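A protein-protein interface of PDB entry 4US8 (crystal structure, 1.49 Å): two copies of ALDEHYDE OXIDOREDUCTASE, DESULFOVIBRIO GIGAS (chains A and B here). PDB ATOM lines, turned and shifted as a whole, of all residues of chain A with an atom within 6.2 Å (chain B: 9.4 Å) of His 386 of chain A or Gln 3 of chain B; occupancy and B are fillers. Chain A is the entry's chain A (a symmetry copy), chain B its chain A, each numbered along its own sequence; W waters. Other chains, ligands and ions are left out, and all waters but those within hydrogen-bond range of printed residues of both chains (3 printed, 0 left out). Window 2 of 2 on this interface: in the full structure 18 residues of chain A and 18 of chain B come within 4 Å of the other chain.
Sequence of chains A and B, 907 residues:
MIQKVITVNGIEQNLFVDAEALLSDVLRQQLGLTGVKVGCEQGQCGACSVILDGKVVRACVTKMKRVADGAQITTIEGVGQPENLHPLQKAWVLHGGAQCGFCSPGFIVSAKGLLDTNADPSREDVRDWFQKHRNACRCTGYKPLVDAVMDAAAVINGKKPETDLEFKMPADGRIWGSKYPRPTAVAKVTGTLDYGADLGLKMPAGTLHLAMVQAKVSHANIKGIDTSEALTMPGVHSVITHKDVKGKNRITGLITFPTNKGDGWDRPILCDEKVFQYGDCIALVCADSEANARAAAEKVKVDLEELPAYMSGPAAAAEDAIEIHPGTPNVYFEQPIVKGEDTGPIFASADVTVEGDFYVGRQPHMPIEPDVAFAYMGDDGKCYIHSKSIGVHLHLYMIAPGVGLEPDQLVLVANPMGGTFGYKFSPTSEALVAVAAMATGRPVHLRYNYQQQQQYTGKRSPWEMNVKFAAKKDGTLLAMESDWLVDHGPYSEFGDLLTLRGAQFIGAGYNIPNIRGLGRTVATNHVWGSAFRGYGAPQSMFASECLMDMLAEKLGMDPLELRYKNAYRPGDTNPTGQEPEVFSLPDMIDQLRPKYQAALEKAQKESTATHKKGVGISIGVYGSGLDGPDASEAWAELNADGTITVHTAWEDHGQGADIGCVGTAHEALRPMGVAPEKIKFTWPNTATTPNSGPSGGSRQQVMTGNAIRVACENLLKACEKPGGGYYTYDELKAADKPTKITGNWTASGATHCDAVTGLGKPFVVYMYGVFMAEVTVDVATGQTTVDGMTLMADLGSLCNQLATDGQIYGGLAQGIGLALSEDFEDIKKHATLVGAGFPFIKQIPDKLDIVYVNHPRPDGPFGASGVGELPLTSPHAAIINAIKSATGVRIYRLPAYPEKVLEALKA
No position is printed for both chains.
Along chain A the printed residues that touch a printed residue of chain B span positions 199 to 386.
Printed residues of chain B that touch a printed residue of chain A: Met 1, Gln 3, Asn 14 and Phe 16.
Hydrophobic or aromatic side chains of chain B within 4 Å of the printed part of chain A: Met 1 and Phe 16.
Among the printed residues, 8 pairs touch across the chains.
Among the printed residues, no Asp or Glu carboxylate lies within 4 Å of a Lys or Arg side-chain nitrogen of the other chain.
NE2 of Gln 3 of chain B lies within hydrogen-bond range of OD1 of Asn 14 of chain B, 2.8 Å away.
The backbone carbonyl oxygen of His 386 of chain A sits at hydrogen-bond distance from the side-chain amide nitrogen of Asn 415 of chain A (3.3 Å).
The backbone NH (N) of Tyr 384 of chain A lies within hydrogen-bond range of the backbone carbonyl oxygen (O) of Tyr 376 of chain A (2.9 Å).
Of the printed residues of chain B, Leu 199 of chain A touches Asn 14 and Phe 16.
No residue of chain B comes within 4 Å of Ala 373 of chain A.
Of chain B, only Phe 16 comes within 4 Å of Phe 374 of chain A.
Of chain B, only Gln 3 (3.6 Å) and Phe 16 (3.5 Å) come within 4 Å of His 386 of chain A.
Ser 387 of chain A touches none of the printed residues of chain B.
Of the printed residues of chain A, Met 1 of chain B touches Tyr 376.
Gln 3 of chain B touches two residues of chain A.
Of the printed residues of chain A, Asn 14 of chain B touches Leu 199.
Of the printed residues of chain A, Phe 16 of chain B touches Leu 199 (3.96 Å), Phe 374 (3.6 Å), Tyr 376 (3.9 Å) and His 386 (3.5 Å).
The nearest residue of chain B that does not touch His 386 of chain A is Asn 14 of chain B (5.5 Å).
The nearest printed residue of chain B that does not touch Tyr 376 of chain A is Ile 2 of chain B (4.5 Å).
Water W2 lies within hydrogen-bond range of the side-chain hydroxyl of Tyr 376 of chain A (2.8 Å) and the backbone NH of Gln 3 of chain B (3.0 Å).
Water W3 lies within hydrogen-bond range of the side-chain amide nitrogen (ND2) of Asn 685 of chain A and the side-chain amide oxygen (OE1) of Gln 3 of chain B.
Asn 14 of chain B touches Leu 199 of chain A.
Leu 199 of chain A touches Phe 16 of chain B (CD2 to CE2, 3.96 Å).
Phe 16 of chain B touches Phe 374 of chain A.
SD of Met 1 of chain B touches CG of Tyr 376 of chain A, 3.6 Å away.
Tyr 376 of chain A touches Gln 3 of chain B.
Tyr 376 of chain A touches Phe 16 of chain B.
OE1 of Gln 3 of chain B touches CE1 of His 386 of chain A, 3.6 Å away.
His 386 of chain A touches Phe 16 of chain B.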
ATOM      1  N   LEU A 199      18.750  17.627 -11.637  1.00  0.00           N
ATOM      2  CA  LEU A 199      19.747  18.616 -11.196  1.00  0.00           C
ATOM      3  C   LEU A 199      19.085  19.709 -10.362  1.00  0.00           C
ATOM      4  O   LEU A 199      19.636  20.142  -9.339  1.00  0.00           O
ATOM      5  CB  LEU A 199      20.534  19.185 -12.391  1.00  0.00           C
ATOM      6  CG  LEU A 199      21.396  18.145 -13.110  1.00  0.00           C
ATOM      7  CD1 LEU A 199      21.917  18.685 -14.433  1.00  0.00           C
ATOM      8  CD2 LEU A 199      22.553  17.635 -12.249  1.00  0.00           C
ATOM      9  N   VAL A 372      13.620  21.997 -19.836  1.00  0.00           N
ATOM     10  CA  VAL A 372      14.138  22.384 -18.531  1.00  0.00           C
ATOM     11  C   VAL A 372      15.527  22.980 -18.714  1.00  0.00           C
ATOM     12  O   VAL A 372      16.291  22.530 -19.574  1.00  0.00           O
ATOM     13  CB  VAL A 372      14.114  21.189 -17.559  1.00  0.00           C
ATOM     14  CG1 VAL A 372      14.860  20.008 -18.137  1.00  0.00           C
ATOM     15  CG2 VAL A 372      14.659  21.564 -16.171  1.00  0.00           C
ATOM     16  N   ALA A 373      15.848  24.001 -17.916  1.00  0.00           N
ATOM     17  CA  ALA A 373      17.152  24.629 -17.969  1.00  0.00           C
ATOM     18  C   ALA A 373      17.407  25.329 -16.637  1.00  0.00           C
ATOM     19  O   ALA A 373      16.479  25.632 -15.880  1.00  0.00           O
ATOM     20  CB  ALA A 373      17.201  25.632 -19.101  1.00  0.00           C
ATOM     21  N   PHE A 374      18.665  25.686 -16.428  1.00  0.00           N
ATOM     22  CA  PHE A 374      19.045  26.486 -15.284  1.00  0.00           C
ATOM     23  C   PHE A 374      20.219  27.360 -15.609  1.00  0.00           C
ATOM     24  O   PHE A 374      20.906  27.123 -16.593  1.00  0.00           O
ATOM     25  CB  PHE A 374      19.230  25.625 -14.014  1.00  0.00           C
ATOM     26  CG  PHE A 374      20.294  24.573 -14.088  1.00  0.00           C
ATOM     27  CD1 PHE A 374      21.596  24.863 -13.695  1.00  0.00           C
ATOM     28  CD2 PHE A 374      19.999  23.293 -14.473  1.00  0.00           C
ATOM     29  CE1 PHE A 374      22.580  23.893 -13.717  1.00  0.00           C
ATOM     30  CE2 PHE A 374      20.974  22.318 -14.493  1.00  0.00           C
ATOM     31  CZ  PHE A 374      22.259  22.601 -14.095  1.00  0.00           C
ATOM     32  N   ALA A 375      20.459  28.369 -14.765  1.00  0.00           N
ATOM     33  CA  ALA A 375      21.559  29.296 -15.002  1.00  0.00           C
ATOM     34  C   ALA A 375      22.035  29.836 -13.685  1.00  0.00           C
ATOM     35  O   ALA A 375      21.298  29.834 -12.684  1.00  0.00           O
ATOM     36  CB  ALA A 375      21.151  30.444 -15.902  1.00  0.00           C
ATOM     37  N   TYR A 376      23.261  30.336 -13.693  1.00  0.00           N
ATOM     38  CA  TYR A 376      23.847  30.929 -12.488  1.00  0.00           C
ATOM     39  C   TYR A 376      25.006  31.826 -12.892  1.00  0.00           C
ATOM     40  O   TYR A 376      25.544  31.706 -13.977  1.00  0.00           O
ATOM     41  CB  TYR A 376      24.314  29.831 -11.496  1.00  0.00           C
ATOM     42  CG  TYR A 376      25.260  28.821 -12.102  1.00  0.00           C
ATOM     43  CD1 TYR A 376      26.633  29.038 -12.097  1.00  0.00           C
ATOM     44  CD2 TYR A 376      24.793  27.663 -12.731  1.00  0.00           C
ATOM     45  CE1 TYR A 376      27.516  28.146 -12.701  1.00  0.00           C
ATOM     46  CE2 TYR A 376      25.670  26.762 -13.326  1.00  0.00           C
ATOM     47  CZ  TYR A 376      27.021  27.007 -13.328  1.00  0.00           C
ATOM     48  OH  TYR A 376      27.858  26.102 -13.927  1.00  0.00           O
ATOM     49  N   TYR A 384      26.527  31.167 -16.620  1.00  0.00           N
ATOM     50  CA  TYR A 384      26.483  29.783 -17.097  1.00  0.00           C
ATOM     51  C   TYR A 384      25.025  29.365 -17.281  1.00  0.00           C
ATOM     52  O   TYR A 384      24.187  29.598 -16.390  1.00  0.00           O
ATOM     53  CB  TYR A 384      27.128  28.855 -16.071  1.00  0.00           C
ATOM     54  CG  TYR A 384      28.624  28.976 -15.996  1.00  0.00           C
ATOM     55  CD1 TYR A 384      29.226  30.057 -15.352  1.00  0.00           C
ATOM     56  CD2 TYR A 384      29.441  28.038 -16.590  1.00  0.00           C
ATOM     57  CE1 TYR A 384      30.596  30.195 -15.309  1.00  0.00           C
ATOM     58  CE2 TYR A 384      30.807  28.165 -16.554  1.00  0.00           C
ATOM     59  CZ  TYR A 384      31.381  29.242 -15.903  1.00  0.00           C
ATOM     60  OH  TYR A 384      32.745  29.339 -15.905  1.00  0.00           O
ATOM     61  N   ILE A 385      24.754  28.713 -18.412  1.00  0.00           N
ATOM     62  CA  ILE A 385      23.441  28.163 -18.719  1.00  0.00           C
ATOM     63  C   ILE A 385      23.633  26.680 -19.012  1.00  0.00           C
ATOM     64  O   ILE A 385      24.492  26.304 -19.817  1.00  0.00           O
ATOM     65  CB  ILE A 385      22.840  28.838 -19.964  1.00  0.00           C
ATOM     66  CG1 ILE A 385      22.702  30.347 -19.775  1.00  0.00           C
ATOM     67  CG2 ILE A 385      21.472  28.213 -20.302  1.00  0.00           C
ATOM     68  CD1 ILE A 385      22.442  31.043 -21.106  1.00  0.00           C
ATOM     69  N   HIS A 386      22.807  25.858 -18.358  1.00  0.00           N
ATOM     70  CA  HIS A 386      22.791  24.408 -18.552  1.00  0.00           C
ATOM     71  C   HIS A 386      21.399  24.039 -19.033  1.00  0.00           C
ATOM     72  O   HIS A 386      20.434  24.286 -18.331  1.00  0.00           O
ATOM     73  CB  HIS A 386      23.133  23.702 -17.247  1.00  0.00           C
ATOM     74  CG  HIS A 386      24.542  23.947 -16.775  1.00  0.00           C
ATOM     75  ND1 HIS A 386      25.509  22.970 -16.757  1.00  0.00           N
ATOM     76  CD2 HIS A 386      25.156  25.072 -16.320  1.00  0.00           C
ATOM     77  CE1 HIS A 386      26.632  23.452 -16.294  1.00  0.00           C
ATOM     78  NE2 HIS A 386      26.463  24.733 -16.033  1.00  0.00           N
ATOM     79  N   SER A 387      21.292  23.508 -20.238  1.00  0.00           N
ATOM     80  CA  SER A 387      19.975  23.307 -20.862  1.00  0.00           C
ATOM     81  C   SER A 387      19.974  22.075 -21.766  1.00  0.00           C
ATOM     82  O   SER A 387      20.962  21.354 -21.852  1.00  0.00           O
ATOM     83  CB  SER A 387      19.552  24.553 -21.643  1.00  0.00           C
ATOM     84  OG  SER A 387      20.251  24.640 -22.866  1.00  0.00           O
ATOM     85  N   LYS A 388      18.887  21.903 -22.505  1.00  0.00           N
ATOM     86  CA  LYS A 388      18.786  20.864 -23.517  1.00  0.00           C
ATOM     87  C   LYS A 388      19.292  21.340 -24.895  1.00  0.00           C
ATOM     88  O   LYS A 388      19.027  20.704 -25.899  1.00  0.00           O
ATOM     89  CB  LYS A 388      17.336  20.362 -23.640  1.00  0.00           C
ATOM     90  CG  LYS A 388      16.799  19.744 -22.354  1.00  0.00           C
ATOM     91  CD  LYS A 388      15.364  19.271 -22.515  1.00  0.00           C
ATOM     92  CE  LYS A 388      15.179  18.281 -23.661  1.00  0.00           C
ATOM     93  NZ  LYS A 388      13.928  17.478 -23.501  1.00  0.00           N
ATOM     94  N   VAL A 411      28.566  31.115 -20.874  1.00  0.00           N
ATOM     95  CA  VAL A 411      28.971  29.729 -21.131  1.00  0.00           C
ATOM     96  C   VAL A 411      27.708  28.877 -21.221  1.00  0.00           C
ATOM     97  O   VAL A 411      26.875  28.946 -20.326  1.00  0.00           O
ATOM     98  CB  VAL A 411      29.851  29.158 -20.001  1.00  0.00           C
ATOM     99  CG1 VAL A 411      30.257  27.709 -20.284  1.00  0.00           C
ATOM    100  CG2 VAL A 411      31.080  30.049 -19.794  1.00  0.00           C
ATOM    101  N   LEU A 412      27.551  28.133 -22.323  1.00  0.00           N
ATOM    102  CA  LEU A 412      26.421  27.200 -22.466  1.00  0.00           C
ATOM    103  C   LEU A 412      26.928  25.770 -22.393  1.00  0.00           C
ATOM    104  O   LEU A 412      27.939  25.409 -22.991  1.00  0.00           O
ATOM    105  CB  LEU A 412      25.623  27.409 -23.754  1.00  0.00           C
ATOM    106  CG  LEU A 412      24.603  28.532 -23.739  1.00  0.00           C
ATOM    107  CD1 LEU A 412      25.236  29.898 -23.618  1.00  0.00           C
ATOM    108  CD2 LEU A 412      23.708  28.463 -24.947  1.00  0.00           C
ATOM    109  N   VAL A 413      26.173  24.977 -21.658  1.00  0.00           N
ATOM    110  CA  VAL A 413      26.461  23.574 -21.396  1.00  0.00           C
ATOM    111  C   VAL A 413      25.193  22.762 -21.711  1.00  0.00           C
ATOM    112  O   VAL A 413      24.070  23.186 -21.382  1.00  0.00           O
ATOM    113  CB  VAL A 413      26.876  23.368 -19.930  1.00  0.00           C
ATOM    114  CG1 VAL A 413      27.138  21.882 -19.672  1.00  0.00           C
ATOM    115  CG2 VAL A 413      28.096  24.230 -19.566  1.00  0.00           C
ATOM    116  N   ALA A 414      25.365  21.601 -22.343  1.00  0.00           N
ATOM    117  CA  ALA A 414      24.243  20.681 -22.617  1.00  0.00           C
ATOM    118  C   ALA A 414      24.168  19.709 -21.452  1.00  0.00           C
ATOM    119  O   ALA A 414      25.110  18.946 -21.203  1.00  0.00           O
ATOM    120  CB  ALA A 414      24.409  19.926 -23.924  1.00  0.00           C
ATOM    121  N   ASN A 415      23.061  19.745 -20.726  1.00  0.00           N
ATOM    122  CA  ASN A 415      22.762  18.688 -19.747  1.00  0.00           C
ATOM    123  C   ASN A 415      22.466  17.369 -20.448  1.00  0.00           C
ATOM    124  O   ASN A 415      22.009  17.366 -21.610  1.00  0.00           O
ATOM    125  CB  ASN A 415      21.495  19.061 -18.968  1.00  0.00           C
ATOM    126  CG  ASN A 415      21.714  20.179 -17.967  1.00  0.00           C
ATOM    127  OD1 ASN A 415      22.770  20.268 -17.345  1.00  0.00           O
ATOM    128  ND2 ASN A 415      20.696  21.005 -17.766  1.00  0.00           N
ATOM    129  N   VAL A 433      16.367  31.948 -18.569  1.00  0.00           N
ATOM    130  CA  VAL A 433      17.119  31.676 -17.348  1.00  0.00           C
ATOM    131  C   VAL A 433      18.338  32.616 -17.219  1.00  0.00           C
ATOM    132  O   VAL A 433      18.672  33.050 -16.114  1.00  0.00           O
ATOM    133  CB  VAL A 433      17.497  30.181 -17.171  1.00  0.00           C
ATOM    134  CG1 VAL A 433      16.248  29.316 -16.964  1.00  0.00           C
ATOM    135  CG2 VAL A 433      18.360  29.632 -18.299  1.00  0.00           C
ATOM    136  N   ASN A 685      30.298  22.049 -23.855  1.00  0.00           N
ATOM    137  CA  ASN A 685      30.528  23.206 -22.997  1.00  0.00           C
ATOM    138  C   ASN A 685      31.242  24.256 -23.850  1.00  0.00           C
ATOM    139  O   ASN A 685      32.331  23.988 -24.387  1.00  0.00           O
ATOM    140  CB  ASN A 685      31.419  22.754 -21.818  1.00  0.00           C
ATOM    141  CG  ASN A 685      31.783  23.884 -20.895  1.00  0.00           C
ATOM    142  OD1 ASN A 685      32.260  24.929 -21.350  1.00  0.00           O
ATOM    143  ND2 ASN A 685      31.627  23.678 -19.609  1.00  0.00           N
ATOM    144  N   MET B   1      28.306  30.455  -7.904  1.00  0.00           N
ATOM    145  CA  MET B   1      28.032  28.985  -7.925  1.00  0.00           C
ATOM    146  C   MET B   1      29.048  28.354  -8.860  1.00  0.00           C
ATOM    147  O   MET B   1      29.546  29.014  -9.795  1.00  0.00           O
ATOM    148  CB  MET B   1      26.599  28.717  -8.435  1.00  0.00           C
ATOM    149  CG  MET B   1      26.337  27.279  -8.910  1.00  0.00           C
ATOM    150  SD  MET B   1      24.596  26.937  -9.164  1.00  0.00           S
ATOM    151  CE  MET B   1      24.054  26.591  -7.520  1.00  0.00           C
ATOM    152  N   ILE B   2      29.344  27.074  -8.663  1.00  0.00           N
ATOM    153  CA  ILE B   2      30.271  26.365  -9.555  1.00  0.00           C
ATOM    154  C   ILE B   2      29.778  24.927  -9.792  1.00  0.00           C
ATOM    155  O   ILE B   2      29.196  24.292  -8.897  1.00  0.00           O
ATOM    156  CB  ILE B   2      31.734  26.406  -9.033  1.00  0.00           C
ATOM    157  CG1 ILE B   2      32.722  25.968 -10.119  1.00  0.00           C
ATOM    158  CG2 ILE B   2      31.920  25.586  -7.763  1.00  0.00           C
ATOM    159  CD1 ILE B   2      34.129  26.410  -9.831  1.00  0.00           C
ATOM    160  N   GLN B   3      30.007  24.438 -11.002  1.00  0.00           N
ATOM    161  CA  GLN B   3      29.847  23.030 -11.332  1.00  0.00           C
ATOM    162  C   GLN B   3      31.108  22.279 -10.910  1.00  0.00           C
ATOM    163  O   GLN B   3      32.216  22.692 -11.227  1.00  0.00           O
ATOM    164  CB  GLN B   3      29.632  22.872 -12.836  1.00  0.00           C
ATOM    165  CG  GLN B   3      29.512  21.431 -13.307  1.00  0.00           C
ATOM    166  CD  GLN B   3      29.401  21.322 -14.820  1.00  0.00           C
ATOM    167  OE1 GLN B   3      29.955  22.159 -15.560  1.00  0.00           O
ATOM    168  NE2 GLN B   3      28.756  20.301 -15.296  1.00  0.00           N
ATOM    169  N   LYS B   4      30.916  21.148 -10.232  1.00  0.00           N
ATOM    170  CA  LYS B   4      32.002  20.235  -9.902  1.00  0.00           C
ATOM    171  C   LYS B   4      31.578  18.834 -10.241  1.00  0.00           C
ATOM    172  O   LYS B   4      30.590  18.335  -9.691  1.00  0.00           O
ATOM    173  CB  LYS B   4      32.307  20.287  -8.421  1.00  0.00           C
ATOM    174  CG  LYS B   4      32.990  21.552  -7.994  1.00  0.00           C
ATOM    175  CD  LYS B   4      33.348  21.398  -6.529  1.00  0.00           C
ATOM    176  CE  LYS B   4      33.953  22.682  -6.042  1.00  0.00           C
ATOM    177  NZ  LYS B   4      35.334  22.861  -6.538  1.00  0.00           N
ATOM    178  N   VAL B   5      32.384  18.176 -11.035  1.00  0.00           N
ATOM    179  CA  VAL B   5      32.119  16.805 -11.460  1.00  0.00           C
ATOM    180  C   VAL B   5      33.069  15.935 -10.647  1.00  0.00           C
ATOM    181  O   VAL B   5      34.297  16.038 -10.782  1.00  0.00           O
ATOM    182  CB  VAL B   5      32.279  16.623 -12.968  1.00  0.00           C
ATOM    183  CG1 VAL B   5      32.082  15.156 -13.342  1.00  0.00           C
ATOM    184  CG2 VAL B   5      31.284  17.535 -13.700  1.00  0.00           C
ATOM    185  N   ILE B   6      32.477  15.155  -9.736  1.00  0.00           N
ATOM    186  CA  ILE B   6      33.237  14.334  -8.785  1.00  0.00           C
ATOM    187  C   ILE B   6      32.616  12.935  -8.724  1.00  0.00           C
ATOM    188  O   ILE B   6      31.598  12.689  -9.377  1.00  0.00           O
ATOM    189  CB  ILE B   6      33.282  14.962  -7.376  1.00  0.00           C
ATOM    190  CG1 ILE B   6      31.895  15.035  -6.733  1.00  0.00           C
ATOM    191  CG2 ILE B   6      33.924  16.362  -7.416  1.00  0.00           C
ATOM    192  CD1 ILE B   6      31.958  15.333  -5.244  1.00  0.00           C
ATOM    193  N   GLU B  12      29.629   8.856 -10.511  1.00  0.00           N
ATOM    194  CA  GLU B  12      29.925  10.213 -10.941  1.00  0.00           C
ATOM    195  C   GLU B  12      28.721  11.111 -10.637  1.00  0.00           C
ATOM    196  O   GLU B  12      27.563  10.773 -10.963  1.00  0.00           O
ATOM    197  CB  GLU B  12      30.236  10.269 -12.453  1.00  0.00           C
ATOM    198  CG  GLU B  12      30.738  11.631 -12.885  1.00  0.00           C
ATOM    199  CD  GLU B  12      31.049  11.725 -14.357  1.00  0.00           C
ATOM    200  OE1 GLU B  12      32.027  11.102 -14.782  1.00  0.00           O
ATOM    201  OE2 GLU B  12      30.316  12.429 -15.098  1.00  0.00           O
ATOM    202  N   GLN B  13      29.016  12.266 -10.071  1.00  0.00           N
ATOM    203  CA  GLN B  13      28.024  13.260  -9.673  1.00  0.00           C
ATOM    204  C   GLN B  13      28.316  14.556 -10.381  1.00  0.00           C
ATOM    205  O   GLN B  13      29.450  15.031 -10.322  1.00  0.00           O
ATOM    206  CB  GLN B  13      28.117  13.559  -8.163  1.00  0.00           C
ATOM    207  CG  GLN B  13      27.760  12.422  -7.244  1.00  0.00           C
ATOM    208  CD  GLN B  13      26.303  12.078  -7.279  1.00  0.00           C
ATOM    209  OE1 GLN B  13      25.435  12.956  -7.293  1.00  0.00           O
ATOM    210  NE2 GLN B  13      26.015  10.780  -7.291  1.00  0.00           N
ATOM    211  N   ASN B  14      27.304  15.131 -11.029  1.00  0.00           N
ATOM    212  CA  ASN B  14      27.406  16.432 -11.678  1.00  0.00           C
ATOM    213  C   ASN B  14      26.843  17.454 -10.694  1.00  0.00           C
ATOM    214  O   ASN B  14      25.637  17.672 -10.641  1.00  0.00           O
ATOM    215  CB  ASN B  14      26.603  16.399 -12.982  1.00  0.00           C
ATOM    216  CG  ASN B  14      26.710  17.675 -13.762  1.00  0.00           C
ATOM    217  OD1 ASN B  14      27.649  18.455 -13.579  1.00  0.00           O
ATOM    218  ND2 ASN B  14      25.765  17.879 -14.681  1.00  0.00           N
ATOM    219  N   LEU B  15      27.710  18.028  -9.855  1.00  0.00           N
ATOM    220  CA  LEU B  15      27.284  18.828  -8.693  1.00  0.00           C
ATOM    221  C   LEU B  15      27.301  20.282  -8.977  1.00  0.00           C
ATOM    222  O   LEU B  15      28.227  20.804  -9.612  1.00  0.00           O
ATOM    223  CB  LEU B  15      28.174  18.624  -7.472  1.00  0.00           C
ATOM    224  CG  LEU B  15      28.177  17.334  -6.748  1.00  0.00           C
ATOM    225  CD1 LEU B  15      29.163  17.487  -5.569  1.00  0.00           C
ATOM    226  CD2 LEU B  15      26.751  17.065  -6.298  1.00  0.00           C
ATOM    227  N   PHE B  16      26.296  20.950  -8.438  1.00  0.00           N
ATOM    228  CA  PHE B  16      26.211  22.404  -8.493  1.00  0.00           C
ATOM    229  C   PHE B  16      26.138  22.952  -7.086  1.00  0.00           C
ATOM    230  O   PHE B  16      25.201  22.670  -6.344  1.00  0.00           O
ATOM    231  CB  PHE B  16      24.980  22.773  -9.314  1.00  0.00           C
ATOM    232  CG  PHE B  16      25.151  22.375 -10.759  1.00  0.00           C
ATOM    233  CD1 PHE B  16      25.780  23.225 -11.650  1.00  0.00           C
ATOM    234  CD2 PHE B  16      24.804  21.104 -11.167  1.00  0.00           C
ATOM    235  CE1 PHE B  16      25.998  22.824 -12.950  1.00  0.00           C
ATOM    236  CE2 PHE B  16      25.059  20.692 -12.458  1.00  0.00           C
ATOM    237  CZ  PHE B  16      25.657  21.550 -13.344  1.00  0.00           C
ATOM    238  N   VAL B  17      27.171  23.692  -6.722  1.00  0.00           N
ATOM    239  CA  VAL B  17      27.377  24.083  -5.346  1.00  0.00           C
ATOM    240  C   VAL B  17      27.893  25.500  -5.215  1.00  0.00           C
ATOM    241  O   VAL B  17      28.484  26.058  -6.142  1.00  0.00           O
ATOM    242  CB  VAL B  17      28.391  23.148  -4.627  1.00  0.00           C
ATOM    243  CG1 VAL B  17      27.825  21.734  -4.485  1.00  0.00           C
ATOM    244  CG2 VAL B  17      29.765  23.133  -5.308  1.00  0.00           C
ATOM    245  N   ASP B  18      27.656  26.062  -4.033  1.00  0.00           N
ATOM    246  CA  ASP B  18      28.360  27.256  -3.602  1.00  0.00           C
ATOM    247  C   ASP B  18      29.741  26.810  -3.070  1.00  0.00           C
ATOM    248  O   ASP B  18      29.856  25.881  -2.268  1.00  0.00           O
ATOM    249  CB  ASP B  18      27.590  28.023  -2.546  1.00  0.00           C
ATOM    250  CG  ASP B  18      28.095  29.436  -2.408  1.00  0.00           C
ATOM    251  OD1 ASP B  18      27.609  30.324  -3.148  1.00  0.00           O
ATOM    252  OD2 ASP B  18      29.014  29.649  -1.589  1.00  0.00           O
ATOM    253  N   ALA B  19      30.789  27.482  -3.515  1.00  0.00           N
ATOM    254  CA  ALA B  19      32.150  27.145  -3.097  1.00  0.00           C
ATOM    255  C   ALA B  19      32.351  27.270  -1.586  1.00  0.00           C
ATOM    256  O   ALA B  19      33.238  26.611  -1.019  1.00  0.00           O
ATOM    257  CB  ALA B  19      33.151  28.004  -3.844  1.00  0.00           C
ATOM    258  N   MET B  64      33.288  23.464   0.033  1.00  0.00           N
ATOM    259  CA  MET B  64      33.373  22.854  -1.297  1.00  0.00           C
ATOM    260  C   MET B  64      34.524  23.337  -2.124  1.00  0.00           C
ATOM    261  O   MET B  64      34.983  22.634  -3.003  1.00  0.00           O
ATOM    262  CB  MET B  64      32.074  23.054  -2.047  1.00  0.00           C
ATOM    263  CG  MET B  64      30.879  22.325  -1.430  1.00  0.00           C
ATOM    264  SD  MET B  64      31.122  20.563  -1.183  1.00  0.00           S
ATOM    265  CE  MET B  64      31.510  20.025  -2.819  1.00  0.00           C
ATOM    266  N   VAL B  67      37.154  20.807  -2.453  1.00  0.00           N
ATOM    267  CA  VAL B  67      36.860  19.591  -3.192  1.00  0.00           C
ATOM    268  C   VAL B  67      37.151  19.848  -4.675  1.00  0.00           C
ATOM    269  O   VAL B  67      36.481  20.652  -5.325  1.00  0.00           O
ATOM    270  CB  VAL B  67      35.399  19.168  -2.992  1.00  0.00           C
ATOM    271  CG1 VAL B  67      35.099  17.861  -3.736  1.00  0.00           C
ATOM    272  CG2 VAL B  67      35.077  19.018  -1.500  1.00  0.00           C
ATOM    273  N   ALA B  68      38.182  19.198  -5.183  1.00  0.00           N
ATOM    274  CA  ALA B  68      38.585  19.455  -6.557  1.00  0.00           C
ATOM    275  C   ALA B  68      37.723  18.698  -7.535  1.00  0.00           C
ATOM    276  O   ALA B  68      37.166  17.657  -7.207  1.00  0.00           O
ATOM    277  CB  ALA B  68      40.031  19.048  -6.755  1.00  0.00           C
ATOM    278  N   ASP B  69      37.639  19.212  -8.765  1.00  0.00           N
ATOM    279  CA  ASP B  69      37.087  18.441  -9.878  1.00  0.00           C
ATOM    280  C   ASP B  69      37.796  17.093  -9.877  1.00  0.00           C
ATOM    281  O   ASP B  69      39.016  17.021  -9.752  1.00  0.00           O
ATOM    282  CB  ASP B  69      37.316  19.097 -11.259  1.00  0.00           C
ATOM    283  CG  ASP B  69      36.139  19.974 -11.751  1.00  0.00           C
ATOM    284  OD1 ASP B  69      34.948  19.571 -11.791  1.00  0.00           O
ATOM    285  OD2 ASP B  69      36.466  21.108 -12.167  1.00  0.00           O
ATOM    286  N   GLY B  70      37.013  16.027 -10.023  1.00  0.00           N
ATOM    287  CA  GLY B  70      37.524  14.672 -10.066  1.00  0.00           C
ATOM    288  C   GLY B  70      37.807  14.049  -8.728  1.00  0.00           C
ATOM    289  O   GLY B  70      38.271  12.900  -8.664  1.00  0.00           O
HETATM  290  O   HOH W   1      25.418  20.096 -16.823  1.00  0.00           O
HETATM  291  O   HOH W   2      30.568  26.184 -13.397  1.00  0.00           O
HETATM  292  O   HOH W   3      30.645  21.392 -18.401  1.00  0.00           O
